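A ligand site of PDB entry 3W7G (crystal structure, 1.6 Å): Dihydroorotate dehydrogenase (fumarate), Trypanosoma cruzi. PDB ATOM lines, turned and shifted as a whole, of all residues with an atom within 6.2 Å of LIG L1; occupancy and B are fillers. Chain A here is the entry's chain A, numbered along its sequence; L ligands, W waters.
N of Met 70 lies close to OD1 of Asn 68 (3.4 Å).
The side-chain amide nitrogen of Asn 54 sits at hydrogen-bond distance from the backbone carbonyl oxygen of Ser 69 (2.9 Å).
The backbone carbonyl oxygen (O) of Met 70 lies within hydrogen-bond range of the backbone NH (N) of Asn 54 (2.9 Å).
The guanidinium group of Arg 51 lies within hydrogen-bond range of the backbone carbonyl oxygen of Leu 72, 3.2 Å away.
ND2 of Asn 128 sits at hydrogen-bond distance from OG of Ser 100 (3.3 Å).
The side-chain amide oxygen (OD1) of Asn 128 is in hydrogen-bond range of the backbone NH (N) of Ser 130, 3.1 Å away.
The side-chain amide nitrogen of Asn 195 lies within hydrogen-bond range of the side-chain amide oxygen of Asn 128 (3.2 Å).
The backbone NH of Gly 71 sits close to the side-chain amide nitrogen of Asn 54 (3.3 Å).
A nitrogen (N2) of LG2 L2 lies close to an oxygen (O4) of LIG L1 (3.4 Å).
Water W1 lies within hydrogen-bond range of an oxygen (O2) of LIG L1, the side-chain amino group of Lys 44 and an oxygen (O2) of LG2 L2.
Water W2 lies within hydrogen-bond range of O1 of LIG L1 (2.7 Å) and O of Asn 68 (2.9 Å).
Water W4 lies within hydrogen-bond range of OG of Ser 196 (2.8 Å) and O3 of LIG L1 (3.2 Å).
The backbone NH (N) of Leu 72 is in hydrogen-bond range of an oxygen (O2) of LIG L1 (2.8 Å).
The side-chain amide nitrogen (ND2) of Asn 195 sits at hydrogen-bond distance from an oxygen (O1) of LG2 L2 (3.2 Å).
The side-chain amino group (NZ) of Lys 165 is in hydrogen-bond range of an oxygen (O3) of LG2 L2 (2.8 Å).
O3 of LIG L1 is in hydrogen-bond range of OG of Ser 196 (2.7 Å).
The side-chain amide oxygen of Asn 68 sits at hydrogen-bond distance from a nitrogen (N1) of LIG L1, at 2.9 Å.
The backbone NH (N) of Gly 71 sits at hydrogen-bond distance from an oxygen (O2) of LIG L1 (3.4 Å).
The side-chain hydroxyl (OG) of Ser 45 lies within hydrogen-bond range of a nitrogen (N2) of LG2 L2 (2.7 Å).
OD1 of Asn 195 lies within hydrogen-bond range of N2 of LIG L1.
The backbone NH (N) of Ala 20 sits at hydrogen-bond distance from an oxygen (O3) of LG2 L2 (3.5 Å).
O4 of LIG L1 lies within hydrogen-bond range of ND2 of Asn 128.
O3 of LG2 L2 sits at hydrogen-bond distance from O of Ala 20, 2.7 Å away.
The backbone NH (N) of Met 70 sits at hydrogen-bond distance from an oxygen (O1) of LIG L1.
Merely in contact with LIG L1: Ser 69 (3.9 Å), Ser 130 (3.6 Å) and Pro 132 (3.4 Å).
Hydrophobic or aromatic side chains that line LIG L1: Met 70, Leu 72 and Pro 132.
Within 4 Å of LIG L1: Asn 68, Ser 69, Met 70, Gly 71, Leu 72, Asn 128, Ser 130, Pro 132, Asn 195 and Ser 196.
The nearest printed residue that does not touch LIG L1 is Leu 102 (4.2 Å).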
ATOM      1  N   ALA A  20      -2.808 -16.133  -1.705  1.00  0.00           N
ATOM      2  CA  ALA A  20      -1.946 -16.410  -0.584  1.00  0.00           C
ATOM      3  C   ALA A  20      -0.794 -17.269  -1.031  1.00  0.00           C
ATOM      4  O   ALA A  20      -0.926 -18.188  -1.782  1.00  0.00           O
ATOM      5  CB  ALA A  20      -2.724 -17.051   0.558  1.00  0.00           C
ATOM      6  N   LYS A  44       1.035 -13.946   3.598  1.00  0.00           N
ATOM      7  CA  LYS A  44       1.379 -15.328   3.520  1.00  0.00           C
ATOM      8  C   LYS A  44       0.728 -16.140   4.648  1.00  0.00           C
ATOM      9  O   LYS A  44       0.864 -15.799   5.827  1.00  0.00           O
ATOM     10  CB  LYS A  44       2.889 -15.484   3.590  1.00  0.00           C
ATOM     11  CG  LYS A  44       3.389 -16.938   3.611  1.00  0.00           C
ATOM     12  CD  LYS A  44       3.104 -17.695   2.346  1.00  0.00           C
ATOM     13  CE  LYS A  44       3.039 -19.185   2.685  1.00  0.00           C
ATOM     14  NZ  LYS A  44       4.261 -19.600   2.096  1.00  0.00           N
ATOM     15  N   SER A  45       0.113 -17.250   4.290  1.00  0.00           N
ATOM     16  CA  SER A  45      -0.467 -18.202   5.292  1.00  0.00           C
ATOM     17  C   SER A  45       0.590 -18.472   6.350  1.00  0.00           C
ATOM     18  O   SER A  45       1.715 -18.853   6.076  1.00  0.00           O
ATOM     19  CB  SER A  45      -0.936 -19.517   4.731  1.00  0.00           C
ATOM     20  OG  SER A  45      -1.945 -19.251   3.771  1.00  0.00           O
ATOM     21  N   ARG A  51       8.491 -20.954   9.995  1.00  0.00           N
ATOM     22  CA  ARG A  51       8.863 -22.174   9.342  1.00  0.00           C
ATOM     23  C   ARG A  51       9.761 -21.863   8.175  1.00  0.00           C
ATOM     24  O   ARG A  51       9.491 -20.979   7.365  1.00  0.00           O
ATOM     25  CB  ARG A  51       7.669 -22.873   8.723  1.00  0.00           C
ATOM     26  CG  ARG A  51       6.695 -23.421   9.784  1.00  0.00           C
ATOM     27  CD  ARG A  51       5.470 -24.033   9.203  1.00  0.00           C
ATOM     28  NE  ARG A  51       5.662 -25.064   8.242  1.00  0.00           N
ATOM     29  CZ  ARG A  51       5.769 -26.339   8.582  1.00  0.00           C
ATOM     30  NH1 ARG A  51       5.689 -26.775   9.843  1.00  0.00           N
ATOM     31  NH2 ARG A  51       5.915 -27.233   7.630  1.00  0.00           N
ATOM     32  N   ASN A  54      10.029 -26.610   3.132  1.00  0.00           N
ATOM     33  CA  ASN A  54      10.691 -27.772   2.571  1.00  0.00           C
ATOM     34  C   ASN A  54      11.930 -27.472   1.800  1.00  0.00           C
ATOM     35  O   ASN A  54      12.213 -26.380   1.394  1.00  0.00           O
ATOM     36  CB  ASN A  54       9.696 -28.435   1.604  1.00  0.00           C
ATOM     37  CG  ASN A  54       8.652 -29.256   2.235  1.00  0.00           C
ATOM     38  OD1 ASN A  54       8.786 -29.704   3.445  1.00  0.00           O
ATOM     39  ND2 ASN A  54       7.495 -29.438   1.579  1.00  0.00           N
ATOM     40  N   ASN A  68       3.958 -26.996  -6.725  1.00  0.00           N
ATOM     41  CA  ASN A  68       4.656 -26.568  -5.515  1.00  0.00           C
ATOM     42  C   ASN A  68       4.357 -27.544  -4.398  1.00  0.00           C
ATOM     43  O   ASN A  68       3.253 -27.969  -4.143  1.00  0.00           O
ATOM     44  CB  ASN A  68       4.352 -25.153  -5.053  1.00  0.00           C
ATOM     45  CG  ASN A  68       3.127 -25.033  -4.211  1.00  0.00           C
ATOM     46  OD1 ASN A  68       3.185 -25.247  -2.975  1.00  0.00           O
ATOM     47  ND2 ASN A  68       2.015 -24.659  -4.814  1.00  0.00           N
ATOM     48  N   SER A  69       5.358 -27.779  -3.589  1.00  0.00           N
ATOM     49  CA  SER A  69       5.257 -28.359  -2.247  1.00  0.00           C
ATOM     50  C   SER A  69       6.170 -27.527  -1.358  1.00  0.00           C
ATOM     51  O   SER A  69       7.236 -27.973  -0.925  1.00  0.00           O
ATOM     52  CB  SER A  69       5.620 -29.842  -2.248  1.00  0.00           C
ATOM     53  OG  SER A  69       4.624 -30.571  -2.925  1.00  0.00           O
ATOM     54  N   MET A  70       5.729 -26.314  -1.012  1.00  0.00           N
ATOM     55  CA  MET A  70       6.549 -25.374  -0.334  1.00  0.00           C
ATOM     56  C   MET A  70       6.878 -25.782   1.087  1.00  0.00           C
ATOM     57  O   MET A  70       7.909 -25.386   1.644  1.00  0.00           O
ATOM     58  CB  MET A  70       5.882 -24.013  -0.306  1.00  0.00           C
ATOM     59  CG  MET A  70       5.603 -23.361  -1.580  1.00  0.00           C
ATOM     60  SD  MET A  70       6.992 -23.099  -2.655  1.00  0.00           S
ATOM     61  CE  MET A  70       7.802 -21.829  -1.821  1.00  0.00           C
ATOM     62  N   GLY A  71       5.967 -26.487   1.754  1.00  0.00           N
ATOM     63  CA  GLY A  71       6.118 -26.780   3.155  1.00  0.00           C
ATOM     64  C   GLY A  71       5.677 -25.714   4.100  1.00  0.00           C
ATOM     65  O   GLY A  71       6.176 -25.601   5.235  1.00  0.00           O
ATOM     66  N   LEU A  72       4.849 -24.817   3.639  1.00  0.00           N
ATOM     67  CA  LEU A  72       4.304 -23.699   4.449  1.00  0.00           C
ATOM     68  C   LEU A  72       5.427 -22.834   5.068  1.00  0.00           C
ATOM     69  O   LEU A  72       5.363 -22.548   6.279  1.00  0.00           O
ATOM     70  CB  LEU A  72       3.320 -24.241   5.483  1.00  0.00           C
ATOM     71  CG  LEU A  72       2.369 -23.301   6.196  1.00  0.00           C
ATOM     72  CD1 LEU A  72       1.824 -22.284   5.263  1.00  0.00           C
ATOM     73  CD2 LEU A  72       1.257 -24.120   6.896  1.00  0.00           C
ATOM     74  N   PRO A  73       6.417 -22.383   4.339  1.00  0.00           N
ATOM     75  CA  PRO A  73       7.401 -21.442   4.870  1.00  0.00           C
ATOM     76  C   PRO A  73       6.708 -20.127   5.202  1.00  0.00           C
ATOM     77  O   PRO A  73       5.815 -19.673   4.492  1.00  0.00           O
ATOM     78  CB  PRO A  73       8.399 -21.303   3.752  1.00  0.00           C
ATOM     79  CG  PRO A  73       7.574 -21.472   2.507  1.00  0.00           C
ATOM     80  CD  PRO A  73       6.559 -22.535   2.866  1.00  0.00           C
ATOM     81  N   SER A 100      -2.879 -20.554   8.559  1.00  0.00           N
ATOM     82  CA  SER A 100      -2.944 -21.937   8.160  1.00  0.00           C
ATOM     83  C   SER A 100      -2.332 -22.853   9.238  1.00  0.00           C
ATOM     84  O   SER A 100      -1.392 -23.535   8.994  1.00  0.00           O
ATOM     85  CB  SER A 100      -2.215 -22.108   6.845  1.00  0.00           C
ATOM     86  OG  SER A 100      -2.301 -23.403   6.374  1.00  0.00           O
ATOM     87  N   LEU A 102      -1.608 -25.911  11.751  1.00  0.00           N
ATOM     88  CA  LEU A 102      -1.489 -27.327  11.411  1.00  0.00           C
ATOM     89  C   LEU A 102      -2.313 -28.187  12.372  1.00  0.00           C
ATOM     90  O   LEU A 102      -2.360 -29.441  12.264  1.00  0.00           O
ATOM     91  CB  LEU A 102       0.025 -27.725  11.362  1.00  0.00           C
ATOM     92  CG  LEU A 102       0.768 -26.977  10.204  1.00  0.00           C
ATOM     93  CD1 LEU A 102       2.206 -27.338  10.151  1.00  0.00           C
ATOM     94  CD2 LEU A 102       0.178 -27.361   8.884  1.00  0.00           C
ATOM     95  N   ASN A 128      -7.104 -20.867   5.982  1.00  0.00           N
ATOM     96  CA  ASN A 128      -6.815 -21.920   5.006  1.00  0.00           C
ATOM     97  C   ASN A 128      -7.265 -23.266   5.492  1.00  0.00           C
ATOM     98  O   ASN A 128      -6.699 -23.812   6.428  1.00  0.00           O
ATOM     99  CB  ASN A 128      -5.334 -21.962   4.684  1.00  0.00           C
ATOM    100  CG  ASN A 128      -5.031 -22.908   3.538  1.00  0.00           C
ATOM    101  OD1 ASN A 128      -5.835 -23.214   2.705  1.00  0.00           O
ATOM    102  ND2 ASN A 128      -3.812 -23.352   3.478  1.00  0.00           N
ATOM    103  N   SER A 130      -7.449 -25.829   3.185  1.00  0.00           N
ATOM    104  CA  SER A 130      -6.651 -26.777   2.224  1.00  0.00           C
ATOM    105  C   SER A 130      -5.177 -27.154   2.652  1.00  0.00           C
ATOM    106  O   SER A 130      -4.339 -26.538   2.225  1.00  0.00           O
ATOM    107  CB  SER A 130      -6.605 -26.242   0.814  1.00  0.00           C
ATOM    108  OG  SER A 130      -5.932 -27.135  -0.100  1.00  0.00           O
ATOM    109  N   CYS A 131      -5.234 -27.628   3.889  1.00  0.00           N
ATOM    110  CA  CYS A 131      -4.168 -27.659   4.816  1.00  0.00           C
ATOM    111  C   CYS A 131      -4.126 -29.096   5.444  1.00  0.00           C
ATOM    112  O   CYS A 131      -5.102 -29.611   5.811  1.00  0.00           O
ATOM    113  CB  CYS A 131      -4.514 -26.676   6.000  1.00  0.00           C
ATOM    114  SG  CYS A 131      -3.012 -26.370   6.944  1.00  0.00           S
ATOM    115  N   PRO A 132      -2.849 -29.641   5.593  1.00  0.00           N
ATOM    116  CA  PRO A 132      -2.793 -30.850   6.430  1.00  0.00           C
ATOM    117  C   PRO A 132      -3.154 -30.654   7.895  1.00  0.00           C
ATOM    118  O   PRO A 132      -2.998 -29.620   8.434  1.00  0.00           O
ATOM    119  CB  PRO A 132      -1.376 -31.336   6.317  1.00  0.00           C
ATOM    120  CG  PRO A 132      -0.550 -30.263   5.893  1.00  0.00           C
ATOM    121  CD  PRO A 132      -1.403 -29.344   5.102  1.00  0.00           C
ATOM    122  N   LYS A 165     -10.369 -20.450   2.726  1.00  0.00           N
ATOM    123  CA  LYS A 165      -9.700 -20.842   1.465  1.00  0.00           C
ATOM    124  C   LYS A 165      -9.965 -22.330   1.321  1.00  0.00           C
ATOM    125  O   LYS A 165      -9.550 -23.131   2.141  1.00  0.00           O
ATOM    126  CB  LYS A 165      -8.238 -20.602   1.597  1.00  0.00           C
ATOM    127  CG  LYS A 165      -7.371 -20.947   0.349  1.00  0.00           C
ATOM    128  CD  LYS A 165      -7.618 -20.025  -0.835  1.00  0.00           C
ATOM    129  CE  LYS A 165      -6.655 -20.197  -1.968  1.00  0.00           C
ATOM    130  NZ  LYS A 165      -5.317 -19.738  -1.614  1.00  0.00           N
ATOM    131  N   ASN A 195      -7.770 -23.260  -3.775  1.00  0.00           N
ATOM    132  CA  ASN A 195      -6.382 -23.626  -3.538  1.00  0.00           C
ATOM    133  C   ASN A 195      -5.900 -24.587  -4.679  1.00  0.00           C
ATOM    134  O   ASN A 195      -6.690 -24.877  -5.597  1.00  0.00           O
ATOM    135  CB  ASN A 195      -6.192 -24.215  -2.105  1.00  0.00           C
ATOM    136  CG  ASN A 195      -4.834 -23.911  -1.503  1.00  0.00           C
ATOM    137  OD1 ASN A 195      -3.808 -24.040  -2.158  1.00  0.00           O
ATOM    138  ND2 ASN A 195      -4.805 -23.438  -0.310  1.00  0.00           N
ATOM    139  N   SER A 196      -4.637 -25.061  -4.608  1.00  0.00           N
ATOM    140  CA  SER A 196      -4.150 -25.869  -5.692  1.00  0.00           C
ATOM    141  C   SER A 196      -4.886 -27.117  -5.889  1.00  0.00           C
ATOM    142  O   SER A 196      -5.511 -27.686  -5.034  1.00  0.00           O
ATOM    143  CB  SER A 196      -2.769 -26.425  -5.420  1.00  0.00           C
ATOM    144  OG  SER A 196      -2.038 -25.777  -4.506  1.00  0.00           O
ATOM    145  N   LYS A 215       8.219 -34.688  -1.374  1.00  0.00           N
ATOM    146  CA  LYS A 215       7.083 -35.560  -1.686  1.00  0.00           C
ATOM    147  C   LYS A 215       7.295 -36.356  -2.966  1.00  0.00           C
ATOM    148  O   LYS A 215       6.351 -36.648  -3.695  1.00  0.00           O
ATOM    149  CB  LYS A 215       5.790 -34.771  -1.735  1.00  0.00           C
ATOM    150  CG  LYS A 215       5.408 -34.215  -0.355  1.00  0.00           C
ATOM    151  CD  LYS A 215       4.159 -33.266  -0.411  1.00  0.00           C
ATOM    152  CE  LYS A 215       2.999 -33.934  -1.134  1.00  0.00           C
ATOM    153  NZ  LYS A 215       1.687 -33.246  -0.909  1.00  0.00           N
ATOM    154  N   GLY A 220       1.116 -29.375  -5.436  1.00  0.00           N
ATOM    155  CA  GLY A 220      -0.147 -28.791  -5.886  1.00  0.00           C
ATOM    156  C   GLY A 220       0.031 -27.980  -7.138  1.00  0.00           C
ATOM    157  O   GLY A 220       1.014 -27.282  -7.366  1.00  0.00           O
HETATM  158  O1  LIG L   1       2.788 -26.403   0.111  1.00  0.00           O
HETATM  159  C1  LIG L   1       2.412 -25.318   0.718  1.00  0.00           C
HETATM  160  O2  LIG L   1       3.063 -24.672   1.514  1.00  0.00           O
HETATM  161  C2  LIG L   1       1.102 -24.825   0.240  1.00  0.00           C
HETATM  162  N1  LIG L   1       0.993 -24.768  -1.130  1.00  0.00           N
HETATM  163  C3  LIG L   1      -0.133 -24.432  -1.775  1.00  0.00           C
HETATM  164  O3  LIG L   1      -0.265 -24.434  -3.015  1.00  0.00           O
HETATM  165  N2  LIG L   1      -1.227 -24.157  -1.002  1.00  0.00           N
HETATM  166  C4  LIG L   1      -1.222 -24.197   0.415  1.00  0.00           C
HETATM  167  O4  LIG L   1      -2.242 -23.911   1.029  1.00  0.00           O
HETATM  168  C5  LIG L   1      -0.003 -24.517   1.002  1.00  0.00           C
HETATM  169  C6  LIG L   1       0.091 -24.609   2.446  1.00  0.00           C
HETATM  170  C7  LIG L   1      -0.640 -25.856   3.041  1.00  0.00           C
HETATM  171  C8  LIG L   1      -0.055 -27.118   2.597  1.00  0.00           C
HETATM  172  C9  LIG L   1      -0.480 -27.834   1.427  1.00  0.00           C
HETATM  173  C10 LIG L   1       0.164 -29.039   1.023  1.00  0.00           C
HETATM  174  C11 LIG L   1       1.190 -29.588   1.743  1.00  0.00           C
HETATM  175  C12 LIG L   1       1.621 -28.947   2.871  1.00  0.00           C
HETATM  176  C13 LIG L   1       0.998 -27.763   3.324  1.00  0.00           C
HETATM  177  O5  LIG L   1       1.343 -27.059   4.434  1.00  0.00           O
HETATM  178  C14 LIG L   1       2.360 -27.704   5.334  1.00  0.00           C
HETATM  179  N1  LG2 L   2      -2.529 -20.997  -0.778  1.00  0.00           N
HETATM  180  C1  LG2 L   2      -2.766 -20.752   0.550  1.00  0.00           C
HETATM  181  O1  LG2 L   2      -3.975 -20.532   0.875  1.00  0.00           O
HETATM  182  N2  LG2 L   2      -1.787 -20.559   1.428  1.00  0.00           N
HETATM  183  C2  LG2 L   2      -0.484 -20.652   1.062  1.00  0.00           C
HETATM  184  O2  LG2 L   2       0.460 -20.470   1.866  1.00  0.00           O
HETATM  185  C3  LG2 L   2      -0.169 -20.908  -0.271  1.00  0.00           C
HETATM  186  N3  LG2 L   2       1.135 -20.926  -0.680  1.00  0.00           N
HETATM  187  C4  LG2 L   2       1.399 -21.046  -2.033  1.00  0.00           C
HETATM  188  C5  LG2 L   2       2.685 -20.866  -2.497  1.00  0.00           C
HETATM  189  C6  LG2 L   2       2.978 -20.944  -3.835  1.00  0.00           C
HETATM  190  C7  LG2 L   2       4.434 -20.818  -4.323  1.00  0.00           C
HETATM  191  C8  LG2 L   2       1.920 -21.108  -4.787  1.00  0.00           C
HETATM  192  C9  LG2 L   2       2.152 -21.218  -6.265  1.00  0.00           C
HETATM  193  C10 LG2 L   2       0.635 -21.243  -4.320  1.00  0.00           C
HETATM  194  C11 LG2 L   2       0.313 -21.169  -2.974  1.00  0.00           C
HETATM  195  N4  LG2 L   2      -1.004 -21.299  -2.495  1.00  0.00           N
HETATM  196  C12 LG2 L   2      -1.278 -21.025  -1.194  1.00  0.00           C
HETATM  197  C13 LG2 L   2      -2.086 -21.444  -3.435  1.00  0.00           C
HETATM  198  C14 LG2 L   2      -2.499 -20.204  -4.191  1.00  0.00           C
HETATM  199  O3  LG2 L   2      -3.003 -19.283  -3.213  1.00  0.00           O
HETATM  200  C15 LG2 L   2      -3.565 -20.508  -5.181  1.00  0.00           C
HETATM  201  O4  LG2 L   2      -4.732 -20.997  -4.500  1.00  0.00           O
HETATM  202  C16 LG2 L   2      -3.164 -21.547  -6.244  1.00  0.00           C
HETATM  203  O5  LG2 L   2      -1.803 -21.304  -6.696  1.00  0.00           O
HETATM  204  C17 LG2 L   2      -4.098 -21.444  -7.481  1.00  0.00           C
HETATM  205  O6  LG2 L   2      -4.111 -20.175  -8.120  1.00  0.00           O
HETATM  206  P1  LG2 L   2      -3.264 -19.906  -9.478  1.00  0.00           P
HETATM  207  O7  LG2 L   2      -3.443 -18.422  -9.752  1.00  0.00           O
HETATM  208  O8  LG2 L   2      -3.808 -20.853 -10.517  1.00  0.00           O
HETATM  209  O9  LG2 L   2      -1.783 -20.264  -9.125  1.00  0.00           O
HETATM  210  O   HOH W   1       2.962 -22.072   1.535  1.00  0.00           O
HETATM  211  O   HOH W   2       1.517 -27.809  -1.815  1.00  0.00           O
HETATM  212  O   HOH W   3      -3.326 -27.237  -0.476  1.00  0.00           O
HETATM  213  O   HOH W   4      -1.229 -27.390  -2.312  1.00  0.00           O
HETATM  214  O   HOH W   5       4.297 -28.697   0.744  1.00  0.00           O
